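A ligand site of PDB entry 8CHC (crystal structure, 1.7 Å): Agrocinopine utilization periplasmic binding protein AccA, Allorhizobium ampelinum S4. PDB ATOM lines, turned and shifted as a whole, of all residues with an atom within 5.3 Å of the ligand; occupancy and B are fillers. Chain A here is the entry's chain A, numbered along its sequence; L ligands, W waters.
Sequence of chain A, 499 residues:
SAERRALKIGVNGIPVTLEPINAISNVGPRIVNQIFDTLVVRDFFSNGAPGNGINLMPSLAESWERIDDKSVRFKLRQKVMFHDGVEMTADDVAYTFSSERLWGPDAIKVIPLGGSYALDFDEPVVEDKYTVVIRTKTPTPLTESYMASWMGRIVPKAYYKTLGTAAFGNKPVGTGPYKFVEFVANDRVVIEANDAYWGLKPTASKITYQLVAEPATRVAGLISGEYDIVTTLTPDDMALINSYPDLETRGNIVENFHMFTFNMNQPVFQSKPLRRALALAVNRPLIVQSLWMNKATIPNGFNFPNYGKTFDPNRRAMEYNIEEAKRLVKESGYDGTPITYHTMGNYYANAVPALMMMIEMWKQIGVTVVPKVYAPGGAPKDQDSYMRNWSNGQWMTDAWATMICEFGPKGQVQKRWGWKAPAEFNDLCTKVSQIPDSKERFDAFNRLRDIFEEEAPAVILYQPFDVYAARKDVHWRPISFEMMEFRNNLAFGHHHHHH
An oxygen (O9) of the ligand sits close to the backbone NH (N) of Ser 391, at 3.5 Å.
An oxygen (O9) of the ligand sits at hydrogen-bond distance from the side-chain hydroxyl (OG) of Ser 391 (2.6 Å).
The side-chain carboxylate (OE2) of Glu 406 sits at hydrogen-bond distance from an oxygen (O4) of the ligand, 2.7 Å away.
The side-chain hydroxyl (OH) of Tyr 347 lies within hydrogen-bond range of an oxygen (O10) of the ligand.
OH of Tyr 117 lies within hydrogen-bond range of O4 of the ligand (2.7 Å).
OH of Tyr 348 sits at hydrogen-bond distance from O9 of the ligand (2.8 Å).
The backbone NH (N) of Gly 393 is in hydrogen-bond range of an oxygen (O5) of the ligand (2.9 Å).
N of Asn 26 lies within hydrogen-bond range of O10 of the ligand, 2.9 Å away.
An oxygen (O3) of the ligand sits at hydrogen-bond distance from the indole nitrogen of Trp 390 (3.1 Å).
ND2 of Asn 392 sits close to O6 of the ligand (3.2 Å).
The side-chain amide oxygen (OD1) of Asn 26 sits at hydrogen-bond distance from the side-chain hydroxyl (OG) of Ser 391.
ND2 of Asn 256 lies within hydrogen-bond range of OG of Ser 391 (3.2 Å).
OE2 of Glu 406 lies within hydrogen-bond range of OH of Tyr 117.
The side-chain carboxylate of Glu 406 sits at hydrogen-bond distance from the side-chain amide nitrogen of Gln 412, at 3.0 Å.
N of Gly 393 lies close to ND2 of Asn 256.
The side-chain amide oxygen of Asn 392 sits at hydrogen-bond distance from the side-chain hydroxyl of Thr 402 (2.6 Å).
The backbone NH of Val 27 sits at hydrogen-bond distance from the side-chain hydroxyl of Ser 25 (3.2 Å).
CG1 of Val 16 touches O13 of the ligand, 3.9 Å away.
Ile 24 touches the ligand.
Ser 25 touches the ligand.
Trp 150 touches the ligand (CH2 to O1, 3.4 Å).
Thr 402 touches the ligand.
Hydrophobic or aromatic side chains within 4 Å of the ligand: Val 16, Tyr 117, Trp 150, Tyr 347, Tyr 348 and Trp 390.
Within 4 Å of the ligand: Val 16, Ile 24, Ser 25, Asn 26, Tyr 117, Trp 150, Tyr 347, Tyr 348, Trp 390, Ser 391, Asn 392, Gly 393, Thr 402 and Glu 406.
Along chain A the residues within 4 Å of the ligand span positions 16 to 406.
The nearest printed residue that does not touch the ligand is Trp 395 (4.2 Å).
Water W1 lies within hydrogen-bond range of O1 of the ligand (2.8 Å), OD1 of Asn 26 (2.9 Å) and ND2 of Asn 256 (3.3 Å).
Water W3 bridges OH of Tyr 347 and O14 of the ligand.
Water W2 lies within hydrogen-bond range of NE1 of Trp 395 (2.9 Å) and OE2 of Glu 406 (2.9 Å).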
ATOM      1  N   VAL A  16     -28.164 -20.223  28.144  1.00  0.00           N
ATOM      2  CA  VAL A  16     -28.859 -21.372  27.533  1.00  0.00           C
ATOM      3  C   VAL A  16     -29.164 -22.492  28.541  1.00  0.00           C
ATOM      4  O   VAL A  16     -29.979 -23.366  28.263  1.00  0.00           O
ATOM      5  CB  VAL A  16     -28.102 -21.923  26.281  1.00  0.00           C
ATOM      6  CG1 VAL A  16     -28.019 -20.871  25.180  1.00  0.00           C
ATOM      7  CG2 VAL A  16     -26.706 -22.448  26.638  1.00  0.00           C
ATOM      8  N   ILE A  24     -21.251 -20.527  31.767  1.00  0.00           N
ATOM      9  CA  ILE A  24     -20.154 -19.561  31.730  1.00  0.00           C
ATOM     10  C   ILE A  24     -20.316 -18.770  30.441  1.00  0.00           C
ATOM     11  O   ILE A  24     -20.326 -19.338  29.343  1.00  0.00           O
ATOM     12  CB  ILE A  24     -18.730 -20.168  31.837  1.00  0.00           C
ATOM     13  CG1 ILE A  24     -18.498 -20.722  33.253  1.00  0.00           C
ATOM     14  CG2 ILE A  24     -17.657 -19.102  31.496  1.00  0.00           C
ATOM     15  CD1 ILE A  24     -17.277 -21.580  33.415  1.00  0.00           C
ATOM     16  N   SER A  25     -20.489 -17.472  30.618  1.00  0.00           N
ATOM     17  CA  SER A  25     -20.840 -16.494  29.586  1.00  0.00           C
ATOM     18  C   SER A  25     -20.965 -15.098  30.246  1.00  0.00           C
ATOM     19  O   SER A  25     -20.771 -14.964  31.456  1.00  0.00           O
ATOM     20  CB  SER A  25     -22.194 -16.890  28.967  1.00  0.00           C
ATOM     21  OG  SER A  25     -23.235 -16.681  29.916  1.00  0.00           O
ATOM     22  N   ASN A  26     -21.262 -14.065  29.478  1.00  0.00           N
ATOM     23  CA  ASN A  26     -21.495 -12.733  30.036  1.00  0.00           C
ATOM     24  C   ASN A  26     -22.817 -12.670  30.850  1.00  0.00           C
ATOM     25  O   ASN A  26     -22.930 -11.808  31.706  1.00  0.00           O
ATOM     26  CB  ASN A  26     -21.540 -11.676  28.915  1.00  0.00           C
ATOM     27  CG  ASN A  26     -20.180 -11.286  28.371  1.00  0.00           C
ATOM     28  OD1 ASN A  26     -19.127 -11.705  28.858  1.00  0.00           O
ATOM     29  ND2 ASN A  26     -20.164 -10.475  27.318  1.00  0.00           N
ATOM     30  N   VAL A  27     -23.792 -13.573  30.583  1.00  0.00           N
ATOM     31  CA  VAL A  27     -25.133 -13.513  31.146  1.00  0.00           C
ATOM     32  C   VAL A  27     -25.493 -14.619  32.178  1.00  0.00           C
ATOM     33  O   VAL A  27     -26.481 -14.477  32.892  1.00  0.00           O
ATOM     34  CB  VAL A  27     -26.169 -13.490  30.002  1.00  0.00           C
ATOM     35  CG1 VAL A  27     -25.931 -12.279  29.091  1.00  0.00           C
ATOM     36  CG2 VAL A  27     -26.129 -14.779  29.174  1.00  0.00           C
ATOM     37  N   LEU A 113     -16.412 -27.727  27.276  1.00  0.00           N
ATOM     38  CA  LEU A 113     -15.246 -26.911  27.624  1.00  0.00           C
ATOM     39  C   LEU A 113     -14.593 -27.309  28.973  1.00  0.00           C
ATOM     40  O   LEU A 113     -13.566 -26.733  29.337  1.00  0.00           O
ATOM     41  CB  LEU A 113     -15.643 -25.411  27.584  1.00  0.00           C
ATOM     42  CG  LEU A 113     -15.880 -24.707  26.188  1.00  0.00           C
ATOM     43  CD1 LEU A 113     -16.431 -25.625  25.103  1.00  0.00           C
ATOM     44  CD2 LEU A 113     -16.857 -23.538  26.322  1.00  0.00           C
ATOM     45  N   TYR A 117     -10.916 -25.927  30.329  1.00  0.00           N
ATOM     46  CA  TYR A 117     -10.953 -24.998  31.474  1.00  0.00           C
ATOM     47  C   TYR A 117     -10.509 -25.676  32.776  1.00  0.00           C
ATOM     48  O   TYR A 117     -10.431 -24.985  33.774  1.00  0.00           O
ATOM     49  CB  TYR A 117     -12.377 -24.443  31.664  1.00  0.00           C
ATOM     50  CG  TYR A 117     -12.975 -23.629  30.523  1.00  0.00           C
ATOM     51  CD1 TYR A 117     -12.239 -23.323  29.380  1.00  0.00           C
ATOM     52  CD2 TYR A 117     -14.310 -23.214  30.571  1.00  0.00           C
ATOM     53  CE1 TYR A 117     -12.823 -22.660  28.301  1.00  0.00           C
ATOM     54  CE2 TYR A 117     -14.883 -22.518  29.501  1.00  0.00           C
ATOM     55  CZ  TYR A 117     -14.127 -22.230  28.385  1.00  0.00           C
ATOM     56  OH  TYR A 117     -14.704 -21.507  27.353  1.00  0.00           O
ATOM     57  N   TRP A 150     -15.472 -19.065  38.494  1.00  0.00           N
ATOM     58  CA  TRP A 150     -16.711 -19.600  37.962  1.00  0.00           C
ATOM     59  C   TRP A 150     -16.649 -21.102  37.604  1.00  0.00           C
ATOM     60  O   TRP A 150     -17.678 -21.689  37.227  1.00  0.00           O
ATOM     61  CB  TRP A 150     -17.193 -18.758  36.778  1.00  0.00           C
ATOM     62  CG  TRP A 150     -16.208 -18.522  35.680  1.00  0.00           C
ATOM     63  CD1 TRP A 150     -15.046 -19.199  35.424  1.00  0.00           C
ATOM     64  CD2 TRP A 150     -16.321 -17.523  34.666  1.00  0.00           C
ATOM     65  NE1 TRP A 150     -14.486 -18.726  34.252  1.00  0.00           N
ATOM     66  CE2 TRP A 150     -15.222 -17.665  33.799  1.00  0.00           C
ATOM     67  CE3 TRP A 150     -17.276 -16.542  34.376  1.00  0.00           C
ATOM     68  CZ2 TRP A 150     -15.037 -16.859  32.694  1.00  0.00           C
ATOM     69  CZ3 TRP A 150     -17.084 -15.732  33.282  1.00  0.00           C
ATOM     70  CH2 TRP A 150     -15.961 -15.871  32.478  1.00  0.00           C
ATOM     71  N   ASN A 256     -12.358  -8.192  31.013  1.00  0.00           N
ATOM     72  CA  ASN A 256     -12.958  -8.885  29.884  1.00  0.00           C
ATOM     73  C   ASN A 256     -12.640  -8.077  28.636  1.00  0.00           C
ATOM     74  O   ASN A 256     -12.573  -6.845  28.714  1.00  0.00           O
ATOM     75  CB  ASN A 256     -14.496  -8.946  30.081  1.00  0.00           C
ATOM     76  CG  ASN A 256     -15.264  -9.547  28.925  1.00  0.00           C
ATOM     77  OD1 ASN A 256     -15.477  -8.882  27.902  1.00  0.00           O
ATOM     78  ND2 ASN A 256     -15.700 -10.805  29.033  1.00  0.00           N
ATOM     79  N   MET A 344     -25.614 -11.343  17.781  1.00  0.00           N
ATOM     80  CA  MET A 344     -26.905 -11.493  18.443  1.00  0.00           C
ATOM     81  C   MET A 344     -27.345 -10.098  18.964  1.00  0.00           C
ATOM     82  O   MET A 344     -27.353  -9.848  20.152  1.00  0.00           O
ATOM     83  CB  MET A 344     -26.741 -12.510  19.586  1.00  0.00           C
ATOM     84  CG  MET A 344     -28.050 -12.898  20.235  1.00  0.00           C
ATOM     85  SD  MET A 344     -28.021 -14.473  21.101  1.00  0.00           S
ATOM     86  CE  MET A 344     -26.808 -14.174  22.293  1.00  0.00           C
ATOM     87  N   TYR A 347     -26.084  -7.915  22.382  1.00  0.00           N
ATOM     88  CA  TYR A 347     -25.765  -8.810  23.499  1.00  0.00           C
ATOM     89  C   TYR A 347     -24.428  -8.303  24.096  1.00  0.00           C
ATOM     90  O   TYR A 347     -24.307  -8.192  25.310  1.00  0.00           O
ATOM     91  CB  TYR A 347     -25.629 -10.258  22.970  1.00  0.00           C
ATOM     92  CG  TYR A 347     -25.109 -11.248  23.980  1.00  0.00           C
ATOM     93  CD1 TYR A 347     -23.752 -11.480  24.116  1.00  0.00           C
ATOM     94  CD2 TYR A 347     -25.973 -12.023  24.734  1.00  0.00           C
ATOM     95  CE1 TYR A 347     -23.256 -12.411  25.028  1.00  0.00           C
ATOM     96  CE2 TYR A 347     -25.501 -12.970  25.631  1.00  0.00           C
ATOM     97  CZ  TYR A 347     -24.143 -13.143  25.794  1.00  0.00           C
ATOM     98  OH  TYR A 347     -23.683 -14.126  26.639  1.00  0.00           O
ATOM     99  N   TYR A 348     -23.465  -7.917  23.216  1.00  0.00           N
ATOM    100  CA  TYR A 348     -22.254  -7.221  23.604  1.00  0.00           C
ATOM    101  C   TYR A 348     -22.592  -5.735  23.405  1.00  0.00           C
ATOM    102  O   TYR A 348     -23.085  -5.357  22.332  1.00  0.00           O
ATOM    103  CB  TYR A 348     -21.037  -7.594  22.726  1.00  0.00           C
ATOM    104  CG  TYR A 348     -20.677  -9.051  22.788  1.00  0.00           C
ATOM    105  CD1 TYR A 348     -20.268  -9.637  23.979  1.00  0.00           C
ATOM    106  CD2 TYR A 348     -20.834  -9.876  21.690  1.00  0.00           C
ATOM    107  CE1 TYR A 348     -19.975 -10.996  24.057  1.00  0.00           C
ATOM    108  CE2 TYR A 348     -20.520 -11.225  21.750  1.00  0.00           C
ATOM    109  CZ  TYR A 348     -20.137 -11.794  22.946  1.00  0.00           C
ATOM    110  OH  TYR A 348     -19.858 -13.132  23.008  1.00  0.00           O
ATOM    111  N   ASN A 389     -18.716 -12.066  16.561  1.00  0.00           N
ATOM    112  CA  ASN A 389     -18.158 -11.357  17.704  1.00  0.00           C
ATOM    113  C   ASN A 389     -18.165 -12.319  18.903  1.00  0.00           C
ATOM    114  O   ASN A 389     -18.869 -13.332  18.899  1.00  0.00           O
ATOM    115  CB  ASN A 389     -18.842 -10.006  17.973  1.00  0.00           C
ATOM    116  CG  ASN A 389     -20.332 -10.065  18.119  1.00  0.00           C
ATOM    117  OD1 ASN A 389     -20.912 -11.142  18.244  1.00  0.00           O
ATOM    118  ND2 ASN A 389     -20.965  -8.913  18.096  1.00  0.00           N
ATOM    119  N   TRP A 390     -17.299 -12.035  19.859  1.00  0.00           N
ATOM    120  CA  TRP A 390     -17.168 -12.833  21.074  1.00  0.00           C
ATOM    121  C   TRP A 390     -16.506 -11.941  22.153  1.00  0.00           C
ATOM    122  O   TRP A 390     -16.195 -10.765  21.907  1.00  0.00           O
ATOM    123  CB  TRP A 390     -16.336 -14.131  20.768  1.00  0.00           C
ATOM    124  CG  TRP A 390     -16.361 -15.235  21.794  1.00  0.00           C
ATOM    125  CD1 TRP A 390     -17.391 -15.573  22.635  1.00  0.00           C
ATOM    126  CD2 TRP A 390     -15.346 -16.236  21.996  1.00  0.00           C
ATOM    127  NE1 TRP A 390     -17.036 -16.662  23.398  1.00  0.00           N
ATOM    128  CE2 TRP A 390     -15.786 -17.091  23.034  1.00  0.00           C
ATOM    129  CE3 TRP A 390     -14.087 -16.470  21.427  1.00  0.00           C
ATOM    130  CZ2 TRP A 390     -15.023 -18.169  23.483  1.00  0.00           C
ATOM    131  CZ3 TRP A 390     -13.331 -17.540  21.878  1.00  0.00           C
ATOM    132  CH2 TRP A 390     -13.796 -18.362  22.913  1.00  0.00           C
ATOM    133  N   SER A 391     -16.411 -12.473  23.356  1.00  0.00           N
ATOM    134  CA  SER A 391     -15.691 -11.842  24.448  1.00  0.00           C
ATOM    135  C   SER A 391     -14.994 -12.933  25.245  1.00  0.00           C
ATOM    136  O   SER A 391     -15.408 -14.088  25.185  1.00  0.00           O
ATOM    137  CB  SER A 391     -16.632 -11.013  25.328  1.00  0.00           C
ATOM    138  OG  SER A 391     -17.274 -11.757  26.363  1.00  0.00           O
ATOM    139  N   ASN A 392     -13.980 -12.563  26.040  1.00  0.00           N
ATOM    140  CA  ASN A 392     -13.341 -13.487  26.976  1.00  0.00           C
ATOM    141  C   ASN A 392     -13.137 -12.808  28.314  1.00  0.00           C
ATOM    142  O   ASN A 392     -12.393 -11.834  28.390  1.00  0.00           O
ATOM    143  CB  ASN A 392     -11.979 -13.905  26.470  1.00  0.00           C
ATOM    144  CG  ASN A 392     -11.883 -15.130  25.577  1.00  0.00           C
ATOM    145  OD1 ASN A 392     -10.767 -15.631  25.368  1.00  0.00           O
ATOM    146  ND2 ASN A 392     -12.973 -15.643  24.981  1.00  0.00           N
ATOM    147  N   GLY A 393     -13.743 -13.350  29.352  1.00  0.00           N
ATOM    148  CA  GLY A 393     -13.497 -12.878  30.707  1.00  0.00           C
ATOM    149  C   GLY A 393     -12.182 -13.444  31.218  1.00  0.00           C
ATOM    150  O   GLY A 393     -11.941 -14.644  31.089  1.00  0.00           O
ATOM    151  N   TRP A 395     -10.523 -14.649  33.870  1.00  0.00           N
ATOM    152  CA  TRP A 395     -10.975 -15.252  35.121  1.00  0.00           C
ATOM    153  C   TRP A 395      -9.892 -15.808  36.068  1.00  0.00           C
ATOM    154  O   TRP A 395     -10.279 -16.367  37.104  1.00  0.00           O
ATOM    155  CB  TRP A 395     -12.020 -16.347  34.801  1.00  0.00           C
ATOM    156  CG  TRP A 395     -11.581 -17.489  33.923  1.00  0.00           C
ATOM    157  CD1 TRP A 395     -11.538 -17.504  32.562  1.00  0.00           C
ATOM    158  CD2 TRP A 395     -11.258 -18.822  34.350  1.00  0.00           C
ATOM    159  NE1 TRP A 395     -11.195 -18.759  32.108  1.00  0.00           N
ATOM    160  CE2 TRP A 395     -11.064 -19.600  33.186  1.00  0.00           C
ATOM    161  CE3 TRP A 395     -11.231 -19.458  35.587  1.00  0.00           C
ATOM    162  CZ2 TRP A 395     -10.749 -20.946  33.236  1.00  0.00           C
ATOM    163  CZ3 TRP A 395     -10.916 -20.805  35.637  1.00  0.00           C
ATOM    164  CH2 TRP A 395     -10.673 -21.528  34.467  1.00  0.00           C
ATOM    165  N   THR A 402      -7.078 -16.239  29.353  1.00  0.00           N
ATOM    166  CA  THR A 402      -7.756 -17.179  28.457  1.00  0.00           C
ATOM    167  C   THR A 402      -6.920 -17.595  27.243  1.00  0.00           C
ATOM    168  O   THR A 402      -7.416 -18.380  26.433  1.00  0.00           O
ATOM    169  CB  THR A 402      -9.119 -16.612  28.039  1.00  0.00           C
ATOM    170  OG1 THR A 402      -8.978 -15.408  27.302  1.00  0.00           O
ATOM    171  CG2 THR A 402     -10.050 -16.414  29.225  1.00  0.00           C
ATOM    172  N   GLU A 406      -8.761 -21.032  26.079  1.00  0.00           N
ATOM    173  CA  GLU A 406      -9.568 -20.837  24.859  1.00  0.00           C
ATOM    174  C   GLU A 406      -8.748 -21.059  23.563  1.00  0.00           C
ATOM    175  O   GLU A 406      -9.295 -21.621  22.606  1.00  0.00           O
ATOM    176  CB  GLU A 406     -10.182 -19.431  24.792  1.00  0.00           C
ATOM    177  CG  GLU A 406     -11.117 -19.065  25.930  1.00  0.00           C
ATOM    178  CD  GLU A 406     -12.468 -19.749  26.010  1.00  0.00           C
ATOM    179  OE1 GLU A 406     -12.735 -20.733  25.272  1.00  0.00           O
ATOM    180  OE2 GLU A 406     -13.266 -19.316  26.877  1.00  0.00           O
ATOM    181  N   GLN A 412     -11.552 -24.705  22.312  1.00  0.00           N
ATOM    182  CA  GLN A 412     -12.578 -24.668  21.244  1.00  0.00           C
ATOM    183  C   GLN A 412     -12.172 -23.889  19.989  1.00  0.00           C
ATOM    184  O   GLN A 412     -12.778 -24.119  18.946  1.00  0.00           O
ATOM    185  CB  GLN A 412     -13.920 -24.136  21.781  1.00  0.00           C
ATOM    186  CG  GLN A 412     -13.905 -22.638  22.149  1.00  0.00           C
ATOM    187  CD  GLN A 412     -15.231 -22.161  22.691  1.00  0.00           C
ATOM    188  OE1 GLN A 412     -16.283 -22.314  22.059  1.00  0.00           O
ATOM    189  NE2 GLN A 412     -15.214 -21.541  23.866  1.00  0.00           N
HETATM  190  C1  LIG L   1     -16.982 -15.028  28.386  1.00  0.00           C
HETATM  191  C2  LIG L   1     -17.532 -15.779  27.180  1.00  0.00           C
HETATM  192  C3  LIG L   1     -17.332 -17.280  27.301  1.00  0.00           C
HETATM  193  C4  LIG L   1     -15.868 -17.608  27.588  1.00  0.00           C
HETATM  194  C5  LIG L   1     -15.391 -16.815  28.804  1.00  0.00           C
HETATM  195  C6  LIG L   1     -13.918 -16.990  29.092  1.00  0.00           C
HETATM  196  O1  LIG L   1     -17.690 -15.218  29.581  1.00  0.00           O
HETATM  197  O2  LIG L   1     -18.970 -15.586  27.136  1.00  0.00           O
HETATM  198  O3  LIG L   1     -17.806 -17.917  26.106  1.00  0.00           O
HETATM  199  O4  LIG L   1     -15.725 -19.008  27.850  1.00  0.00           O
HETATM  200  O5  LIG L   1     -15.617 -15.408  28.606  1.00  0.00           O
HETATM  201  O6  LIG L   1     -13.132 -16.744  27.933  1.00  0.00           O
HETATM  202  C7  LIG L   1     -22.217 -15.807  23.654  1.00  0.00           C
HETATM  203  O7  LIG L   1     -21.447 -15.452  22.535  1.00  0.00           O
HETATM  204  O8  LIG L   1     -20.050 -15.767  24.816  1.00  0.00           O
HETATM  205  C8  LIG L   1     -21.369 -16.395  24.787  1.00  0.00           C
HETATM  206  C9  LIG L   1     -21.001 -17.851  24.517  1.00  0.00           C
HETATM  207  C10 LIG L   1     -22.939 -18.013  22.982  1.00  0.00           C
HETATM  208  C11 LIG L   1     -24.209 -18.722  22.559  1.00  0.00           C
HETATM  209  O9  LIG L   1     -18.755 -13.726  25.562  1.00  0.00           O
HETATM  210  P1  LIG L   1     -19.750 -14.807  25.952  1.00  0.00           P
HETATM  211  O10 LIG L   1     -20.996 -14.266  26.606  1.00  0.00           O
HETATM  212  O11 LIG L   1     -20.335 -18.418  25.644  1.00  0.00           O
HETATM  213  C12 LIG L   1     -22.245 -18.665  24.169  1.00  0.00           C
HETATM  214  O12 LIG L   1     -21.872 -19.993  23.831  1.00  0.00           O
HETATM  215  O13 LIG L   1     -25.158 -18.744  23.611  1.00  0.00           O
HETATM  216  O14 LIG L   1     -23.317 -16.667  23.336  1.00  0.00           O
HETATM  217  O   HOH W   1     -17.477 -12.836  31.001  1.00  0.00           O
HETATM  218  O   HOH W   2     -11.792 -19.682  29.393  1.00  0.00           O
HETATM  219  O   HOH W   3     -24.990 -16.577  26.102  1.00  0.00           O
